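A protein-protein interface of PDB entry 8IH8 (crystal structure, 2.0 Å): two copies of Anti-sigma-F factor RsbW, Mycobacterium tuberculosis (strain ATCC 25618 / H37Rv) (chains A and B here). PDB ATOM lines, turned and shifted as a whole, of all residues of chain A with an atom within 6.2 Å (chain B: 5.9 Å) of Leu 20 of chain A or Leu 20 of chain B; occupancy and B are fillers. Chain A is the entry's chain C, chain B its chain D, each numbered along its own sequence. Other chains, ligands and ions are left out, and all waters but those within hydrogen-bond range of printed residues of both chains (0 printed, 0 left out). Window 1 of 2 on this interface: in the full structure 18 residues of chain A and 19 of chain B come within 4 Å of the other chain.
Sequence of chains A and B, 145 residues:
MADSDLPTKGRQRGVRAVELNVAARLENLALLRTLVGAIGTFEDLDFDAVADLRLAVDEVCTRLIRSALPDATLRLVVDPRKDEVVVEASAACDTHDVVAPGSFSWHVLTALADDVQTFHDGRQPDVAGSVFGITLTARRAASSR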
ATOM      1  N   VAL A  18     -10.330 -26.227  32.798  1.00  0.00           N
ATOM      2  CA  VAL A  18     -11.285 -25.902  31.743  1.00  0.00           C
ATOM      3  C   VAL A  18     -12.606 -26.556  32.090  1.00  0.00           C
ATOM      4  O   VAL A  18     -12.663 -27.777  32.293  1.00  0.00           O
ATOM      5  CB  VAL A  18     -10.816 -26.374  30.362  1.00  0.00           C
ATOM      6  CG1 VAL A  18     -11.871 -25.992  29.303  1.00  0.00           C
ATOM      7  CG2 VAL A  18      -9.452 -25.775  30.034  1.00  0.00           C
ATOM      8  N   GLU A  19     -13.662 -25.752  32.164  1.00  0.00           N
ATOM      9  CA  GLU A  19     -15.007 -26.276  32.348  1.00  0.00           C
ATOM     10  C   GLU A  19     -15.742 -26.293  31.005  1.00  0.00           C
ATOM     11  O   GLU A  19     -15.865 -25.256  30.340  1.00  0.00           O
ATOM     12  CB  GLU A  19     -15.772 -25.456  33.386  1.00  0.00           C
ATOM     13  CG  GLU A  19     -17.102 -26.069  33.743  1.00  0.00           C
ATOM     14  CD  GLU A  19     -17.918 -25.153  34.605  1.00  0.00           C
ATOM     15  OE1 GLU A  19     -17.459 -24.849  35.726  1.00  0.00           O
ATOM     16  OE2 GLU A  19     -18.998 -24.725  34.150  1.00  0.00           O
ATOM     17  N   LEU A  20     -16.225 -27.470  30.612  1.00  0.00           N
ATOM     18  CA  LEU A  20     -16.967 -27.657  29.373  1.00  0.00           C
ATOM     19  C   LEU A  20     -18.396 -28.051  29.729  1.00  0.00           C
ATOM     20  O   LEU A  20     -18.609 -29.003  30.490  1.00  0.00           O
ATOM     21  CB  LEU A  20     -16.315 -28.731  28.499  1.00  0.00           C
ATOM     22  CG  LEU A  20     -14.848 -28.536  28.113  1.00  0.00           C
ATOM     23  CD1 LEU A  20     -13.992 -29.032  29.236  1.00  0.00           C
ATOM     24  CD2 LEU A  20     -14.497 -29.325  26.877  1.00  0.00           C
ATOM     25  N   ASN A  21     -19.366 -27.310  29.201  1.00  0.00           N
ATOM     26  CA  ASN A  21     -20.779 -27.577  29.426  1.00  0.00           C
ATOM     27  C   ASN A  21     -21.439 -27.775  28.072  1.00  0.00           C
ATOM     28  O   ASN A  21     -21.372 -26.885  27.216  1.00  0.00           O
ATOM     29  CB  ASN A  21     -21.456 -26.437  30.190  1.00  0.00           C
ATOM     30  CG  ASN A  21     -20.881 -26.251  31.569  1.00  0.00           C
ATOM     31  OD1 ASN A  21     -21.099 -27.062  32.443  1.00  0.00           O
ATOM     32  ND2 ASN A  21     -20.138 -25.168  31.768  1.00  0.00           N
ATOM     33  N   VAL A  22     -22.043 -28.954  27.869  1.00  0.00           N
ATOM     34  CA  VAL A  22     -22.792 -29.265  26.657  1.00  0.00           C
ATOM     35  C   VAL A  22     -24.072 -29.983  27.059  1.00  0.00           C
ATOM     36  O   VAL A  22     -24.166 -30.568  28.141  1.00  0.00           O
ATOM     37  CB  VAL A  22     -21.999 -30.146  25.667  1.00  0.00           C
ATOM     38  CG1 VAL A  22     -20.755 -29.450  25.191  1.00  0.00           C
ATOM     39  CG2 VAL A  22     -21.656 -31.528  26.301  1.00  0.00           C
ATOM     40  N   LEU A  32     -16.585 -33.375  22.475  1.00  0.00           N
ATOM     41  CA  LEU A  32     -15.913 -33.413  23.771  1.00  0.00           C
ATOM     42  C   LEU A  32     -14.567 -34.122  23.683  1.00  0.00           C
ATOM     43  O   LEU A  32     -13.564 -33.643  24.234  1.00  0.00           O
ATOM     44  CB  LEU A  32     -16.801 -34.105  24.813  1.00  0.00           C
ATOM     45  CG  LEU A  32     -18.013 -33.313  25.299  1.00  0.00           C
ATOM     46  CD1 LEU A  32     -18.863 -34.149  26.262  1.00  0.00           C
ATOM     47  CD2 LEU A  32     -17.567 -32.005  25.933  1.00  0.00           C
ATOM     48  N   LEU A  35     -12.047 -31.817  22.111  1.00  0.00           N
ATOM     49  CA  LEU A  35     -11.598 -30.748  22.990  1.00  0.00           C
ATOM     50  C   LEU A  35     -10.697 -31.297  24.080  1.00  0.00           C
ATOM     51  O   LEU A  35      -9.671 -30.688  24.412  1.00  0.00           O
ATOM     52  CB  LEU A  35     -12.802 -30.017  23.585  1.00  0.00           C
ATOM     53  CG  LEU A  35     -13.694 -29.437  22.493  1.00  0.00           C
ATOM     54  CD1 LEU A  35     -14.866 -28.663  23.051  1.00  0.00           C
ATOM     55  CD2 LEU A  35     -12.875 -28.564  21.572  1.00  0.00           C
ATOM     56  N   VAL A  36     -11.050 -32.458  24.631  1.00  0.00           N
ATOM     57  CA  VAL A  36     -10.230 -33.059  25.677  1.00  0.00           C
ATOM     58  C   VAL A  36      -8.846 -33.399  25.132  1.00  0.00           C
ATOM     59  O   VAL A  36      -7.829 -33.190  25.799  1.00  0.00           O
ATOM     60  CB  VAL A  36     -10.945 -34.296  26.252  1.00  0.00           C
ATOM     61  CG1 VAL A  36      -9.971 -35.188  26.964  1.00  0.00           C
ATOM     62  CG2 VAL A  36     -12.066 -33.854  27.185  1.00  0.00           C
ATOM     63  N   ILE A  39      -6.808 -30.271  24.866  1.00  0.00           N
ATOM     64  CA  ILE A  39      -6.283 -29.854  26.170  1.00  0.00           C
ATOM     65  C   ILE A  39      -5.050 -30.670  26.534  1.00  0.00           C
ATOM     66  O   ILE A  39      -4.021 -30.128  26.959  1.00  0.00           O
ATOM     67  CB  ILE A  39      -7.351 -29.986  27.269  1.00  0.00           C
ATOM     68  CG1 ILE A  39      -8.523 -29.031  27.033  1.00  0.00           C
ATOM     69  CG2 ILE A  39      -6.699 -29.763  28.635  1.00  0.00           C
ATOM     70  CD1 ILE A  39      -9.705 -29.276  27.953  1.00  0.00           C
ATOM     71  N   LEU A  74     -24.493 -31.665  30.564  1.00  0.00           N
ATOM     72  CA  LEU A  74     -23.307 -32.380  31.009  1.00  0.00           C
ATOM     73  C   LEU A  74     -22.213 -31.357  31.296  1.00  0.00           C
ATOM     74  O   LEU A  74     -21.859 -30.562  30.417  1.00  0.00           O
ATOM     75  CB  LEU A  74     -22.857 -33.389  29.956  1.00  0.00           C
ATOM     76  CG  LEU A  74     -21.511 -34.085  30.140  1.00  0.00           C
ATOM     77  CD1 LEU A  74     -21.456 -34.948  31.402  1.00  0.00           C
ATOM     78  CD2 LEU A  74     -21.213 -34.910  28.887  1.00  0.00           C
ATOM     79  N   ARG A  75     -21.707 -31.351  32.531  1.00  0.00           N
ATOM     80  CA  ARG A  75     -20.644 -30.439  32.948  1.00  0.00           C
ATOM     81  C   ARG A  75     -19.373 -31.248  33.159  1.00  0.00           C
ATOM     82  O   ARG A  75     -19.344 -32.159  33.996  1.00  0.00           O
ATOM     83  CB  ARG A  75     -21.017 -29.686  34.221  1.00  0.00           C
ATOM     84  CG  ARG A  75     -19.863 -28.869  34.808  1.00  0.00           C
ATOM     85  CD  ARG A  75     -20.288 -28.063  36.052  1.00  0.00           C
ATOM     86  NE  ARG A  75     -20.815 -26.736  35.725  1.00  0.00           N
ATOM     87  CZ  ARG A  75     -22.098 -26.462  35.493  1.00  0.00           C
ATOM     88  NH1 ARG A  75     -23.018 -27.424  35.541  1.00  0.00           N
ATOM     89  NH2 ARG A  75     -22.460 -25.221  35.198  1.00  0.00           N
ATOM     90  N   LEU A  76     -18.329 -30.914  32.404  1.00  0.00           N
ATOM     91  CA  LEU A  76     -17.061 -31.628  32.435  1.00  0.00           C
ATOM     92  C   LEU A  76     -15.961 -30.652  32.823  1.00  0.00           C
ATOM     93  O   LEU A  76     -15.872 -29.555  32.252  1.00  0.00           O
ATOM     94  CB  LEU A  76     -16.761 -32.233  31.070  1.00  0.00           C
ATOM     95  CG  LEU A  76     -15.369 -32.815  30.840  1.00  0.00           C
ATOM     96  CD1 LEU A  76     -15.180 -34.067  31.739  1.00  0.00           C
ATOM     97  CD2 LEU A  76     -15.246 -33.183  29.415  1.00  0.00           C
ATOM     98  N   VAL A  77     -15.130 -31.036  33.787  1.00  0.00           N
ATOM     99  CA  VAL A  77     -14.007 -30.207  34.230  1.00  0.00           C
ATOM    100  C   VAL A  77     -12.743 -31.009  34.006  1.00  0.00           C
ATOM    101  O   VAL A  77     -12.624 -32.143  34.498  1.00  0.00           O
ATOM    102  CB  VAL A  77     -14.125 -29.796  35.705  1.00  0.00           C
ATOM    103  CG1 VAL A  77     -12.912 -28.942  36.120  1.00  0.00           C
ATOM    104  CG2 VAL A  77     -15.433 -29.068  35.953  1.00  0.00           C
ATOM    105  N   VAL A  78     -11.822 -30.440  33.241  1.00  0.00           N
ATOM    106  CA  VAL A  78     -10.500 -31.009  33.026  1.00  0.00           C
ATOM    107  C   VAL A  78      -9.514 -30.054  33.678  1.00  0.00           C
ATOM    108  O   VAL A  78      -9.377 -28.899  33.249  1.00  0.00           O
ATOM    109  CB  VAL A  78     -10.185 -31.179  31.532  1.00  0.00           C
ATOM    110  CG1 VAL A  78      -8.778 -31.715  31.348  1.00  0.00           C
ATOM    111  CG2 VAL A  78     -11.222 -32.084  30.861  1.00  0.00           C
ATOM    112  N   VAL B  18     -21.461 -25.402  22.795  1.00  0.00           N
ATOM    113  CA  VAL B  18     -20.553 -25.718  23.885  1.00  0.00           C
ATOM    114  C   VAL B  18     -20.222 -24.431  24.627  1.00  0.00           C
ATOM    115  O   VAL B  18     -19.988 -23.388  24.004  1.00  0.00           O
ATOM    116  CB  VAL B  18     -19.275 -26.417  23.384  1.00  0.00           C
ATOM    117  CG1 VAL B  18     -18.533 -25.548  22.389  1.00  0.00           C
ATOM    118  CG2 VAL B  18     -18.372 -26.774  24.556  1.00  0.00           C
ATOM    119  N   GLU B  19     -20.261 -24.489  25.951  1.00  0.00           N
ATOM    120  CA  GLU B  19     -19.815 -23.390  26.794  1.00  0.00           C
ATOM    121  C   GLU B  19     -18.497 -23.796  27.438  1.00  0.00           C
ATOM    122  O   GLU B  19     -18.418 -24.840  28.096  1.00  0.00           O
ATOM    123  CB  GLU B  19     -20.853 -23.048  27.861  1.00  0.00           C
ATOM    124  CG  GLU B  19     -20.388 -21.943  28.830  1.00  0.00           C
ATOM    125  CD  GLU B  19     -21.330 -21.771  30.013  1.00  0.00           C
ATOM    126  OE1 GLU B  19     -22.472 -21.319  29.823  1.00  0.00           O
ATOM    127  OE2 GLU B  19     -20.933 -22.126  31.139  1.00  0.00           O
ATOM    128  N   LEU B  20     -17.468 -22.986  27.236  1.00  0.00           N
ATOM    129  CA  LEU B  20     -16.175 -23.202  27.868  1.00  0.00           C
ATOM    130  C   LEU B  20     -15.948 -22.109  28.904  1.00  0.00           C
ATOM    131  O   LEU B  20     -16.223 -20.934  28.644  1.00  0.00           O
ATOM    132  CB  LEU B  20     -15.045 -23.171  26.838  1.00  0.00           C
ATOM    133  CG  LEU B  20     -15.120 -24.073  25.611  1.00  0.00           C
ATOM    134  CD1 LEU B  20     -14.047 -23.671  24.643  1.00  0.00           C
ATOM    135  CD2 LEU B  20     -14.926 -25.505  26.006  1.00  0.00           C
ATOM    136  N   ASN B  21     -15.426 -22.482  30.066  1.00  0.00           N
ATOM    137  CA  ASN B  21     -15.084 -21.500  31.092  1.00  0.00           C
ATOM    138  C   ASN B  21     -13.675 -21.771  31.590  1.00  0.00           C
ATOM    139  O   ASN B  21     -13.374 -22.893  32.016  1.00  0.00           O
ATOM    140  CB  ASN B  21     -16.061 -21.567  32.274  1.00  0.00           C
ATOM    141  CG  ASN B  21     -17.471 -21.163  31.887  1.00  0.00           C
ATOM    142  OD1 ASN B  21     -17.747 -19.997  31.675  1.00  0.00           O
ATOM    143  ND2 ASN B  21     -18.359 -22.130  31.793  1.00  0.00           N
ATOM    144  N   VAL B  22     -12.828 -20.739  31.558  1.00  0.00           N
ATOM    145  CA  VAL B  22     -11.467 -20.784  32.082  1.00  0.00           C
ATOM    146  C   VAL B  22     -11.202 -19.494  32.854  1.00  0.00           C
ATOM    147  O   VAL B  22     -11.851 -18.472  32.640  1.00  0.00           O
ATOM    148  CB  VAL B  22     -10.417 -20.924  30.968  1.00  0.00           C
ATOM    149  CG1 VAL B  22     -10.717 -22.114  30.097  1.00  0.00           C
ATOM    150  CG2 VAL B  22     -10.369 -19.640  30.139  1.00  0.00           C
ATOM    151  N   LEU B  32      -7.056 -21.105  25.012  1.00  0.00           N
ATOM    152  CA  LEU B  32      -8.305 -20.765  24.345  1.00  0.00           C
ATOM    153  C   LEU B  32      -8.156 -20.874  22.830  1.00  0.00           C
ATOM    154  O   LEU B  32      -9.021 -21.442  22.147  1.00  0.00           O
ATOM    155  CB  LEU B  32      -8.732 -19.363  24.771  1.00  0.00           C
ATOM    156  CG  LEU B  32      -9.286 -19.271  26.194  1.00  0.00           C
ATOM    157  CD1 LEU B  32      -9.370 -17.849  26.714  1.00  0.00           C
ATOM    158  CD2 LEU B  32     -10.658 -19.872  26.205  1.00  0.00           C
ATOM    159  N   LEU B  35      -8.327 -24.446  21.691  1.00  0.00           N
ATOM    160  CA  LEU B  35      -9.695 -24.965  21.730  1.00  0.00           C
ATOM    161  C   LEU B  35     -10.552 -24.394  20.603  1.00  0.00           C
ATOM    162  O   LEU B  35     -11.372 -25.112  20.014  1.00  0.00           O
ATOM    163  CB  LEU B  35     -10.340 -24.630  23.069  1.00  0.00           C
ATOM    164  CG  LEU B  35      -9.614 -25.208  24.276  1.00  0.00           C
ATOM    165  CD1 LEU B  35     -10.283 -24.732  25.547  1.00  0.00           C
ATOM    166  CD2 LEU B  35      -9.644 -26.719  24.171  1.00  0.00           C
ATOM    167  N   VAL B  36     -10.431 -23.090  20.345  1.00  0.00           N
ATOM    168  CA  VAL B  36     -11.197 -22.469  19.254  1.00  0.00           C
ATOM    169  C   VAL B  36     -10.826 -23.099  17.913  1.00  0.00           C
ATOM    170  O   VAL B  36     -11.695 -23.340  17.059  1.00  0.00           O
ATOM    171  CB  VAL B  36     -10.972 -20.941  19.232  1.00  0.00           C
ATOM    172  CG1 VAL B  36     -11.529 -20.318  17.943  1.00  0.00           C
ATOM    173  CG2 VAL B  36     -11.630 -20.277  20.430  1.00  0.00           C
ATOM    174  N   ILE B  39     -12.442 -26.458  17.596  1.00  0.00           N
ATOM    175  CA  ILE B  39     -13.862 -26.385  17.274  1.00  0.00           C
ATOM    176  C   ILE B  39     -14.061 -26.036  15.801  1.00  0.00           C
ATOM    177  O   ILE B  39     -14.890 -26.638  15.109  1.00  0.00           O
ATOM    178  CB  ILE B  39     -14.554 -25.371  18.203  1.00  0.00           C
ATOM    179  CG1 ILE B  39     -14.593 -25.936  19.630  1.00  0.00           C
ATOM    180  CG2 ILE B  39     -15.959 -25.103  17.720  1.00  0.00           C
ATOM    181  CD1 ILE B  39     -15.046 -24.930  20.671  1.00  0.00           C
ATOM    182  N   LEU B  74     -13.422 -16.292  32.217  1.00  0.00           N
ATOM    183  CA  LEU B  74     -13.721 -15.981  30.826  1.00  0.00           C
ATOM    184  C   LEU B  74     -14.659 -17.067  30.315  1.00  0.00           C
ATOM    185  O   LEU B  74     -14.320 -18.252  30.375  1.00  0.00           O
ATOM    186  CB  LEU B  74     -12.449 -15.898  29.988  1.00  0.00           C
ATOM    187  CG  LEU B  74     -12.782 -15.386  28.567  1.00  0.00           C
ATOM    188  CD1 LEU B  74     -11.625 -14.686  27.994  1.00  0.00           C
ATOM    189  CD2 LEU B  74     -13.108 -16.572  27.651  1.00  0.00           C
ATOM    190  N   ARG B  75     -15.857 -16.680  29.888  1.00  0.00           N
ATOM    191  CA  ARG B  75     -16.821 -17.632  29.357  1.00  0.00           C
ATOM    192  C   ARG B  75     -16.839 -17.529  27.842  1.00  0.00           C
ATOM    193  O   ARG B  75     -16.904 -16.427  27.286  1.00  0.00           O
ATOM    194  CB  ARG B  75     -18.221 -17.392  29.925  1.00  0.00           C
ATOM    195  CG  ARG B  75     -19.315 -18.248  29.264  1.00  0.00           C
ATOM    196  CD  ARG B  75     -20.623 -18.172  30.060  1.00  0.00           C
ATOM    197  NE  ARG B  75     -20.374 -18.406  31.483  1.00  0.00           N
ATOM    198  CZ  ARG B  75     -21.255 -18.923  32.334  1.00  0.00           C
ATOM    199  NH1 ARG B  75     -22.477 -19.241  31.922  1.00  0.00           N
ATOM    200  NH2 ARG B  75     -20.919 -19.103  33.606  1.00  0.00           N
ATOM    201  N   LEU B  76     -16.766 -18.673  27.173  1.00  0.00           N
ATOM    202  CA  LEU B  76     -16.761 -18.708  25.717  1.00  0.00           C
ATOM    203  C   LEU B  76     -17.858 -19.666  25.284  1.00  0.00           C
ATOM    204  O   LEU B  76     -17.833 -20.843  25.674  1.00  0.00           O
ATOM    205  CB  LEU B  76     -15.394 -19.162  25.203  1.00  0.00           C
ATOM    206  CG  LEU B  76     -15.046 -18.964  23.738  1.00  0.00           C
ATOM    207  CD1 LEU B  76     -15.162 -17.509  23.386  1.00  0.00           C
ATOM    208  CD2 LEU B  76     -13.645 -19.488  23.494  1.00  0.00           C
ATOM    209  N   VAL B  77     -18.837 -19.169  24.525  1.00  0.00           N
ATOM    210  CA  VAL B  77     -19.943 -20.008  24.050  1.00  0.00           C
ATOM    211  C   VAL B  77     -19.819 -20.097  22.538  1.00  0.00           C
ATOM    212  O   VAL B  77     -19.816 -19.067  21.851  1.00  0.00           O
ATOM    213  CB  VAL B  77     -21.319 -19.437  24.433  1.00  0.00           C
ATOM    214  CG1 VAL B  77     -22.472 -20.286  23.803  1.00  0.00           C
ATOM    215  CG2 VAL B  77     -21.457 -19.284  25.926  1.00  0.00           C
ATOM    216  N   VAL B  78     -19.699 -21.310  22.016  1.00  0.00           N
ATOM    217  CA  VAL B  78     -19.626 -21.534  20.577  1.00  0.00           C
ATOM    218  C   VAL B  78     -20.889 -22.263  20.158  1.00  0.00           C
ATOM    219  O   VAL B  78     -21.188 -23.348  20.673  1.00  0.00           O
ATOM    220  CB  VAL B  78     -18.367 -22.319  20.188  1.00  0.00           C
ATOM    221  CG1 VAL B  78     -18.301 -22.470  18.676  1.00  0.00           C
ATOM    222  CG2 VAL B  78     -17.160 -21.577  20.684  1.00  0.00           C
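OE2 of Glu 19 of chain A sits at hydrogen-bond distance from ND2 of Asn 21 of chain A, at 2.7 Å. The side-chain carboxylate (OE2) of Glu 19 of chain A lies within salt-bridge range of the guanidinium group (NE) of Arg 75 of chain A (3.1 Å). The backbone carbonyl oxygen (O) of Leu 76 of chain A sits at hydrogen-bond distance from the backbone NH (N) of Leu 20 of chain A, at 2.7 Å. O of Val 22 of chain A lies within hydrogen-bond range of N of Leu 74 of chain A. The side-chain amide nitrogen (ND2) of Asn 21 of chain B sits at hydrogen-bond distance from the side-chain carboxylate (OE2) of Glu 19 of chain B (2.7 Å). The side-chain amide oxygen (OD1) of Asn 21 of chain B is in hydrogen-bond range of the guanidinium group (NE) of Arg 75 of chain B (3.1 Å).
The backbone carbonyl oxygen of Glu 19 of chain A is in hydrogen-bond range of the backbone NH of Asn 21 of chain B (2.8 Å). N of Asn 21 of chain A lies within hydrogen-bond range of O of Glu 19 of chain B. The backbone carbonyl oxygen (O) of Glu 19 of chain B lies close to the backbone carbonyl oxygen (O) of Glu 19 of chain A, at 3.4 Å.
Printed residues of chain A that touch a printed residue of chain B: Val 18, Glu 19, Leu 20, Asn 21, Val 22, Leu 35 and Ile 39. Hydrophobic or aromatic side chains of chain A that line the printed part of chain B: Val 18, Leu 20, Val 22, Leu 35 and Ile 39. Of the 14 printed residues of chain B, 7 touch a printed residue of chain A. Printed residues of chain B that touch a printed residue of chain A: Val 18, Glu 19, Leu 20, Asn 21, Val 22, Leu 35 and Ile 39. Hydrophobic or aromatic side chains of chain B that line the printed part of chain A: Val 18, Leu 20, Val 22, Leu 35 and Ile 39. Among the printed residues, no Asp or Glu carboxylate lies within 4 Å of a Lys or Arg side-chain nitrogen of the other chain.
Printed residues of chain B within 4 Å of Val 18 of chain A: Asn 21 (3.7 Å) and Val 22 (3.9 Å). Leu 20 of chain A touches just these residues of chain B: Glu 19 (3.4 Å) and Leu 20 (3.7 Å). Of the printed residues of chain B, Asn 21 of chain A touches Val 18, Glu 19 and Asn 21. Arg 75 of chain A touches none of the printed residues of chain B. Val 78 of chain A touches none of the printed residues of chain B. Leu 20 of chain B touches just these residues of chain A: Glu 19 and Leu 20. Printed residues of chain A within 4 Å of Val 22 of chain B: Val 18. Printed residues of chain A within 4 Å of Leu 35 of chain B: Leu 35 and Ile 39. The nearest residue of chain B that does not touch Leu 20 of chain A is Val 18 of chain B (4.9 Å). The nearest residue of chain A that does not touch Leu 20 of chain B is Leu 35 of chain A (4.3 Å).
Val 18 of chain A touches Asn 21 of chain B, and with the chains exchanged Asn 21 of chain A touches Val 18 of chain B. Val 18 of chain A touches Val 22 of chain B, and with the chains exchanged Val 22 of chain A touches Val 18 of chain B. Asn 21 of chain A touches its own counterpart, Asn 21 of chain B. Leu 35 of chain A touches Ile 39 of chain B, and with the chains exchanged Ile 39 of chain A touches Leu 35 of chain B.
Val 18 of chain A touches Asn 21 of chain B (CA to O, 3.7 Å). Val 18 of chain A touches Val 22 of chain B. O of Glu 19 of chain A touches CA of Leu 20 of chain B, 3.2 Å away. Glu 19 of chain B touches Leu 20 of chain A (O to CA, 3.4 Å). O of Asn 21 of chain A touches CA of Val 18 of chain B, 3.6 Å away. Asn 21 of chain A touches Asn 21 of chain B. Val 22 of chain A touches Val 18 of chain B. Leu 35 of chain A touches Leu 35 of chain B. Ile 39 of chain B touches Leu 35 of chain A. Ile 39 of chain A touches Leu 35 of chain B.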
